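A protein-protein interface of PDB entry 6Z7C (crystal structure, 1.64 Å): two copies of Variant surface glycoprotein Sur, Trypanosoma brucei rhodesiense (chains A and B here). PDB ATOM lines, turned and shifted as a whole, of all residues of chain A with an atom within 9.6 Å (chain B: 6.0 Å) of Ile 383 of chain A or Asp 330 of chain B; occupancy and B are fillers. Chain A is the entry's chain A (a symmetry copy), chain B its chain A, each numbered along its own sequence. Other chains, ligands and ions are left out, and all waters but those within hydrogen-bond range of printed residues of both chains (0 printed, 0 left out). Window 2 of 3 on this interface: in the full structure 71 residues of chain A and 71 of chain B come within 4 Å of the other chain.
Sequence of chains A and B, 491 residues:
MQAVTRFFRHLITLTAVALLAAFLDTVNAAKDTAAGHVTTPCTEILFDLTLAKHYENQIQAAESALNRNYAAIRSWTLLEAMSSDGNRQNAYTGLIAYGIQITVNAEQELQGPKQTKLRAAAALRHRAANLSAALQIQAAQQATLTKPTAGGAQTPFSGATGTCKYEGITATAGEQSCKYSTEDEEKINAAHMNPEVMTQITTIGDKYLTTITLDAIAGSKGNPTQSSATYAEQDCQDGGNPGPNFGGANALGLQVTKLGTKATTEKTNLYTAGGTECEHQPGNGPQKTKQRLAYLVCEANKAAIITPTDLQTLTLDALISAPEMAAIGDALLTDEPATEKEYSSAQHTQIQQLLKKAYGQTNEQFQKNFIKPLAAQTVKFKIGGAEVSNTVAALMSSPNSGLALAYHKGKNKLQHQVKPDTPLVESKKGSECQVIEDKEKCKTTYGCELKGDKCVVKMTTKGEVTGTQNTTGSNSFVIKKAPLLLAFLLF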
ATOM      1  N   LYS A 380      21.009   0.217 -23.109  1.00  0.00           N
ATOM      2  CA  LYS A 380      19.745   0.665 -23.673  1.00  0.00           C
ATOM      3  C   LYS A 380      18.989  -0.528 -24.240  1.00  0.00           C
ATOM      4  O   LYS A 380      19.591  -1.416 -24.850  1.00  0.00           O
ATOM      5  CB  LYS A 380      19.967   1.724 -24.762  1.00  0.00           C
ATOM      6  N   PHE A 381      17.673  -0.544 -24.027  1.00  0.00           N
ATOM      7  CA  PHE A 381      16.796  -1.591 -24.545  1.00  0.00           C
ATOM      8  C   PHE A 381      15.351  -1.186 -24.279  1.00  0.00           C
ATOM      9  O   PHE A 381      15.078  -0.178 -23.623  1.00  0.00           O
ATOM     10  CB  PHE A 381      17.102  -2.957 -23.920  1.00  0.00           C
ATOM     11  CG  PHE A 381      16.791  -3.037 -22.453  1.00  0.00           C
ATOM     12  CD1 PHE A 381      17.632  -2.454 -21.519  1.00  0.00           C
ATOM     13  CD2 PHE A 381      15.664  -3.706 -22.008  1.00  0.00           C
ATOM     14  CE1 PHE A 381      17.347  -2.528 -20.171  1.00  0.00           C
ATOM     15  CE2 PHE A 381      15.375  -3.786 -20.660  1.00  0.00           C
ATOM     16  CZ  PHE A 381      16.217  -3.194 -19.740  1.00  0.00           C
ATOM     17  N   LYS A 382      14.425  -1.992 -24.798  1.00  0.00           N
ATOM     18  CA  LYS A 382      12.999  -1.740 -24.626  1.00  0.00           C
ATOM     19  C   LYS A 382      12.252  -3.063 -24.683  1.00  0.00           C
ATOM     20  O   LYS A 382      12.400  -3.820 -25.646  1.00  0.00           O
ATOM     21  CB  LYS A 382      12.472  -0.781 -25.701  1.00  0.00           C
ATOM     22  N   ILE A 383      11.454  -3.336 -23.654  1.00  0.00           N
ATOM     23  CA  ILE A 383      10.698  -4.580 -23.577  1.00  0.00           C
ATOM     24  C   ILE A 383       9.378  -4.354 -22.852  1.00  0.00           C
ATOM     25  O   ILE A 383       8.764  -3.294 -22.975  1.00  0.00           O
ATOM     26  CB  ILE A 383      11.512  -5.692 -22.886  1.00  0.00           C
ATOM     27  CG1 ILE A 383      10.633  -6.919 -22.643  1.00  0.00           C
ATOM     28  CG2 ILE A 383      12.091  -5.191 -21.574  1.00  0.00           C
ATOM     29  CD1 ILE A 383      11.413  -8.181 -22.391  1.00  0.00           C
ATOM     30  N   VAL A 388      14.209   1.814 -21.872  1.00  0.00           N
ATOM     31  CA  VAL A 388      15.200   1.890 -20.804  1.00  0.00           C
ATOM     32  C   VAL A 388      16.573   2.254 -21.359  1.00  0.00           C
ATOM     33  O   VAL A 388      17.057   1.632 -22.304  1.00  0.00           O
ATOM     34  CB  VAL A 388      15.274   0.569 -20.017  1.00  0.00           C
ATOM     35  CG1 VAL A 388      16.353   0.646 -18.947  1.00  0.00           C
ATOM     36  CG2 VAL A 388      13.926   0.249 -19.397  1.00  0.00           C
ATOM     37  N   SER A 389      17.194   3.269 -20.765  1.00  0.00           N
ATOM     38  CA  SER A 389      18.536   3.691 -21.152  1.00  0.00           C
ATOM     39  C   SER A 389      19.213   4.281 -19.926  1.00  0.00           C
ATOM     40  O   SER A 389      18.766   5.308 -19.408  1.00  0.00           O
ATOM     41  CB  SER A 389      18.489   4.710 -22.293  1.00  0.00           C
ATOM     42  OG  SER A 389      19.793   5.040 -22.742  1.00  0.00           O
ATOM     43  N   ASN A 400      14.422  -1.032 -13.052  1.00  0.00           N
ATOM     44  CA  ASN A 400      14.601  -1.928 -14.185  1.00  0.00           C
ATOM     45  C   ASN A 400      15.834  -2.812 -14.042  1.00  0.00           C
ATOM     46  O   ASN A 400      16.283  -3.403 -15.029  1.00  0.00           O
ATOM     47  CB  ASN A 400      14.671  -1.122 -15.482  1.00  0.00           C
ATOM     48  CG  ASN A 400      13.448  -0.258 -15.689  1.00  0.00           C
ATOM     49  OD1 ASN A 400      12.337  -0.763 -15.844  1.00  0.00           O
ATOM     50  ND2 ASN A 400      13.644   1.054 -15.691  1.00  0.00           N
ATOM     51  N   GLY A 402      16.367  -5.840 -12.432  1.00  0.00           N
ATOM     52  CA  GLY A 402      16.105  -7.228 -12.773  1.00  0.00           C
ATOM     53  C   GLY A 402      15.717  -7.414 -14.227  1.00  0.00           C
ATOM     54  O   GLY A 402      16.106  -8.398 -14.862  1.00  0.00           O
ATOM     55  N   LEU A 403      14.951  -6.471 -14.780  1.00  0.00           N
ATOM     56  CA  LEU A 403      14.525  -6.609 -16.168  1.00  0.00           C
ATOM     57  C   LEU A 403      15.691  -6.442 -17.135  1.00  0.00           C
ATOM     58  O   LEU A 403      15.711  -7.078 -18.195  1.00  0.00           O
ATOM     59  CB  LEU A 403      13.421  -5.602 -16.483  1.00  0.00           C
ATOM     60  CG  LEU A 403      12.833  -5.670 -17.891  1.00  0.00           C
ATOM     61  CD1 LEU A 403      12.401  -7.095 -18.226  1.00  0.00           C
ATOM     62  CD2 LEU A 403      11.664  -4.711 -18.010  1.00  0.00           C
ATOM     63  N   ALA A 404      16.669  -5.602 -16.789  1.00  0.00           N
ATOM     64  CA  ALA A 404      17.865  -5.487 -17.617  1.00  0.00           C
ATOM     65  C   ALA A 404      18.649  -6.791 -17.626  1.00  0.00           C
ATOM     66  O   ALA A 404      19.166  -7.206 -18.670  1.00  0.00           O
ATOM     67  CB  ALA A 404      18.745  -4.342 -17.121  1.00  0.00           C
ATOM     68  N   LEU A 405      18.748  -7.449 -16.471  1.00  0.00           N
ATOM     69  CA  LEU A 405      19.453  -8.722 -16.403  1.00  0.00           C
ATOM     70  C   LEU A 405      18.753  -9.782 -17.244  1.00  0.00           C
ATOM     71  O   LEU A 405      19.398 -10.509 -18.010  1.00  0.00           O
ATOM     72  CB  LEU A 405      19.570  -9.169 -14.945  1.00  0.00           C
ATOM     73  CG  LEU A 405      20.155 -10.558 -14.691  1.00  0.00           C
ATOM     74  CD1 LEU A 405      21.565 -10.666 -15.272  1.00  0.00           C
ATOM     75  CD2 LEU A 405      20.145 -10.870 -13.194  1.00  0.00           C
ATOM     76  N   ALA A 406      17.425  -9.875 -17.125  1.00  0.00           N
ATOM     77  CA  ALA A 406      16.675 -10.882 -17.872  1.00  0.00           C
ATOM     78  C   ALA A 406      16.755 -10.635 -19.372  1.00  0.00           C
ATOM     79  O   ALA A 406      16.848 -11.585 -20.159  1.00  0.00           O
ATOM     80  CB  ALA A 406      15.216 -10.904 -17.412  1.00  0.00           C
ATOM     81  N   TYR A 407      16.716  -9.366 -19.786  1.00  0.00           N
ATOM     82  CA  TYR A 407      16.801  -9.046 -21.207  1.00  0.00           C
ATOM     83  C   TYR A 407      18.103  -9.560 -21.809  1.00  0.00           C
ATOM     84  O   TYR A 407      18.100 -10.232 -22.846  1.00  0.00           O
ATOM     85  CB  TYR A 407      16.667  -7.535 -21.408  1.00  0.00           C
ATOM     86  CG  TYR A 407      16.860  -7.085 -22.839  1.00  0.00           C
ATOM     87  CD1 TYR A 407      15.821  -7.158 -23.756  1.00  0.00           C
ATOM     88  CD2 TYR A 407      18.083  -6.586 -23.272  1.00  0.00           C
ATOM     89  CE1 TYR A 407      15.995  -6.749 -25.066  1.00  0.00           C
ATOM     90  CE2 TYR A 407      18.266  -6.176 -24.582  1.00  0.00           C
ATOM     91  CZ  TYR A 407      17.218  -6.258 -25.473  1.00  0.00           C
ATOM     92  OH  TYR A 407      17.394  -5.851 -26.779  1.00  0.00           O
ATOM     93  N   HIS A 408      19.233  -9.271 -21.160  1.00  0.00           N
ATOM     94  CA  HIS A 408      20.514  -9.657 -21.738  1.00  0.00           C
ATOM     95  C   HIS A 408      20.832 -11.129 -21.515  1.00  0.00           C
ATOM     96  O   HIS A 408      21.515 -11.739 -22.345  1.00  0.00           O
ATOM     97  CB  HIS A 408      21.627  -8.774 -21.181  1.00  0.00           C
ATOM     98  CG  HIS A 408      21.499  -7.339 -21.583  1.00  0.00           C
ATOM     99  ND1 HIS A 408      20.850  -6.404 -20.806  1.00  0.00           N
ATOM    100  CD2 HIS A 408      21.911  -6.685 -22.695  1.00  0.00           C
ATOM    101  CE1 HIS A 408      20.882  -5.232 -21.416  1.00  0.00           C
ATOM    102  NE2 HIS A 408      21.521  -5.375 -22.563  1.00  0.00           N
ATOM    103  N   LYS A 409      20.355 -11.717 -20.423  1.00  0.00           N
ATOM    104  CA  LYS A 409      20.489 -13.159 -20.238  1.00  0.00           C
ATOM    105  C   LYS A 409      19.559 -13.893 -21.197  1.00  0.00           C
ATOM    106  O   LYS A 409      20.009 -14.671 -22.033  1.00  0.00           O
ATOM    107  CB  LYS A 409      20.189 -13.560 -18.791  1.00  0.00           C
ATOM    108  CG  LYS A 409      21.427 -13.720 -17.908  1.00  0.00           C
ATOM    109  CD  LYS A 409      22.203 -14.991 -18.249  1.00  0.00           C
ATOM    110  CE  LYS A 409      23.465 -15.132 -17.401  1.00  0.00           C
ATOM    111  NZ  LYS A 409      23.190 -15.175 -15.936  1.00  0.00           N
ATOM    112  N   MET B 325       6.828 -10.327 -13.837  1.00  0.00           N
ATOM    113  CA  MET B 325       7.199 -11.535 -14.565  1.00  0.00           C
ATOM    114  C   MET B 325       6.738 -11.527 -16.015  1.00  0.00           C
ATOM    115  O   MET B 325       7.139 -12.414 -16.777  1.00  0.00           O
ATOM    116  CB  MET B 325       6.643 -12.772 -13.860  1.00  0.00           C
ATOM    117  CG  MET B 325       7.395 -13.132 -12.597  1.00  0.00           C
ATOM    118  SD  MET B 325       9.163 -13.325 -12.901  1.00  0.00           S
ATOM    119  CE  MET B 325       9.180 -14.739 -13.996  1.00  0.00           C
ATOM    120  N   ALA B 326       5.909 -10.561 -16.413  1.00  0.00           N
ATOM    121  CA  ALA B 326       5.476 -10.489 -17.804  1.00  0.00           C
ATOM    122  C   ALA B 326       6.647 -10.155 -18.717  1.00  0.00           C
ATOM    123  O   ALA B 326       6.948 -10.898 -19.657  1.00  0.00           O
ATOM    124  CB  ALA B 326       4.355  -9.457 -17.952  1.00  0.00           C
ATOM    125  N   ALA B 327       7.335  -9.044 -18.442  1.00  0.00           N
ATOM    126  CA  ALA B 327       8.477  -8.661 -19.265  1.00  0.00           C
ATOM    127  C   ALA B 327       9.672  -9.578 -19.034  1.00  0.00           C
ATOM    128  O   ALA B 327      10.428  -9.852 -19.969  1.00  0.00           O
ATOM    129  CB  ALA B 327       8.863  -7.208 -18.991  1.00  0.00           C
ATOM    130  N   ILE B 328       9.859 -10.057 -17.803  1.00  0.00           N
ATOM    131  CA  ILE B 328      10.973 -10.958 -17.524  1.00  0.00           C
ATOM    132  C   ILE B 328      10.792 -12.271 -18.273  1.00  0.00           C
ATOM    133  O   ILE B 328      11.706 -12.746 -18.957  1.00  0.00           O
ATOM    134  CB  ILE B 328      11.113 -11.178 -16.007  1.00  0.00           C
ATOM    135  CG1 ILE B 328      11.575  -9.888 -15.326  1.00  0.00           C
ATOM    136  CG2 ILE B 328      12.081 -12.315 -15.720  1.00  0.00           C
ATOM    137  CD1 ILE B 328      11.524  -9.951 -13.806  1.00  0.00           C
ATOM    138  N   GLY B 329       9.604 -12.871 -18.166  1.00  0.00           N
ATOM    139  CA  GLY B 329       9.341 -14.097 -18.900  1.00  0.00           C
ATOM    140  C   GLY B 329       9.436 -13.903 -20.400  1.00  0.00           C
ATOM    141  O   GLY B 329       9.967 -14.756 -21.115  1.00  0.00           O
ATOM    142  N   ASP B 330       8.923 -12.777 -20.898  1.00  0.00           N
ATOM    143  CA  ASP B 330       9.076 -12.461 -22.312  1.00  0.00           C
ATOM    144  C   ASP B 330      10.547 -12.398 -22.701  1.00  0.00           C
ATOM    145  O   ASP B 330      10.926 -12.811 -23.803  1.00  0.00           O
ATOM    146  CB  ASP B 330       8.380 -11.139 -22.624  1.00  0.00           C
ATOM    147  CG  ASP B 330       8.485 -10.760 -24.083  1.00  0.00           C
ATOM    148  OD1 ASP B 330       8.667 -11.666 -24.926  1.00  0.00           O
ATOM    149  OD2 ASP B 330       8.395  -9.553 -24.385  1.00  0.00           O
ATOM    150  N   ALA B 331      11.393 -11.899 -21.798  1.00  0.00           N
ATOM    151  CA  ALA B 331      12.812 -11.754 -22.108  1.00  0.00           C
ATOM    152  C   ALA B 331      13.523 -13.100 -22.122  1.00  0.00           C
ATOM    153  O   ALA B 331      14.418 -13.324 -22.944  1.00  0.00           O
ATOM    154  CB  ALA B 331      13.475 -10.815 -21.100  1.00  0.00           C
ATOM    155  N   LEU B 332      13.141 -14.009 -21.228  1.00  0.00           N
ATOM    156  CA  LEU B 332      13.871 -15.257 -21.055  1.00  0.00           C
ATOM    157  C   LEU B 332      13.193 -16.459 -21.694  1.00  0.00           C
ATOM    158  O   LEU B 332      13.859 -17.478 -21.911  1.00  0.00           O
ATOM    159  CB  LEU B 332      14.085 -15.548 -19.567  1.00  0.00           C
ATOM    160  CG  LEU B 332      15.091 -14.637 -18.868  1.00  0.00           C
ATOM    161  CD1 LEU B 332      14.928 -14.736 -17.369  1.00  0.00           C
ATOM    162  CD2 LEU B 332      16.504 -15.003 -19.275  1.00  0.00           C
ATOM    163  N   LEU B 333      11.902 -16.374 -21.991  1.00  0.00           N
ATOM    164  CA  LEU B 333      11.181 -17.514 -22.534  1.00  0.00           C
ATOM    165  C   LEU B 333      10.699 -17.214 -23.950  1.00  0.00           C
ATOM    166  O   LEU B 333      10.153 -18.080 -24.628  1.00  0.00           O
ATOM    167  CB  LEU B 333      10.003 -17.877 -21.626  1.00  0.00           C
ATOM    168  CG  LEU B 333      10.237 -17.727 -20.117  1.00  0.00           C
ATOM    169  CD1 LEU B 333       8.971 -18.051 -19.332  1.00  0.00           C
ATOM    170  CD2 LEU B 333      11.394 -18.587 -19.639  1.00  0.00           C
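Among the printed residues, merely in contact across the chains: Ile 383 of chain A with Ala 327 of chain B, Ala 406 of chain A with Leu 332 of chain B, Ala 406 of chain A with Ala 331 of chain B, Ile 383 of chain A with Ala 331 of chain B, Leu 403 of chain A with Ala 327 of chain B, Tyr 407 of chain A with Ala 331 of chain B, Lys 409 of chain A with Leu 332 of chain B, Ala 406 of chain A with Ile 328 of chain B, Ile 383 of chain A with Asp 330 of chain B and Leu 403 of chain A with Ile 328 of chain B.
Ile 383 of chain A touches just these residues of chain B: Ala 327 (3.1 Å), Asp 330 (3.9 Å) and Ala 331 (3.6 Å).
Printed residues of chain B within 4 Å of Lys 409 of chain A: Leu 332 (3.8 Å).
Of chain A, only Ile 383 (3.1 Å) and Leu 403 (3.6 Å) come within 4 Å of Ala 327 of chain B.
Of the printed residues of chain A, Ile 328 of chain B touches Leu 403 and Ala 406.
Asp 330 of chain B touches just one residue of chain A: Ile 383 (3.9 Å).
Of the printed residues of chain A, Ala 331 of chain B touches Ile 383 (3.6 Å), Ala 406 (3.6 Å) and Tyr 407 (3.8 Å).
The nearest residue of chain B that does not touch Ile 383 of chain A is Ile 328 of chain B (5.2 Å).
The nearest residue of chain A that does not touch Asp 330 of chain B is Ala 406 of chain A (6.8 Å).
Of the 15 printed residues of chain A, 5 touch a printed residue of chain B.
Printed residues of chain A that touch a printed residue of chain B: Ile 383, Leu 403, Ala 406, Tyr 407 and Lys 409.
Hydrophobic or aromatic side chains of chain A that line the printed part of chain B: Ile 383, Leu 403 and Ala 406.
Among the printed residues, no Asp or Glu carboxylate lies within 4 Å of a Lys or Arg side-chain nitrogen of the other chain.
No position is printed for both chains.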
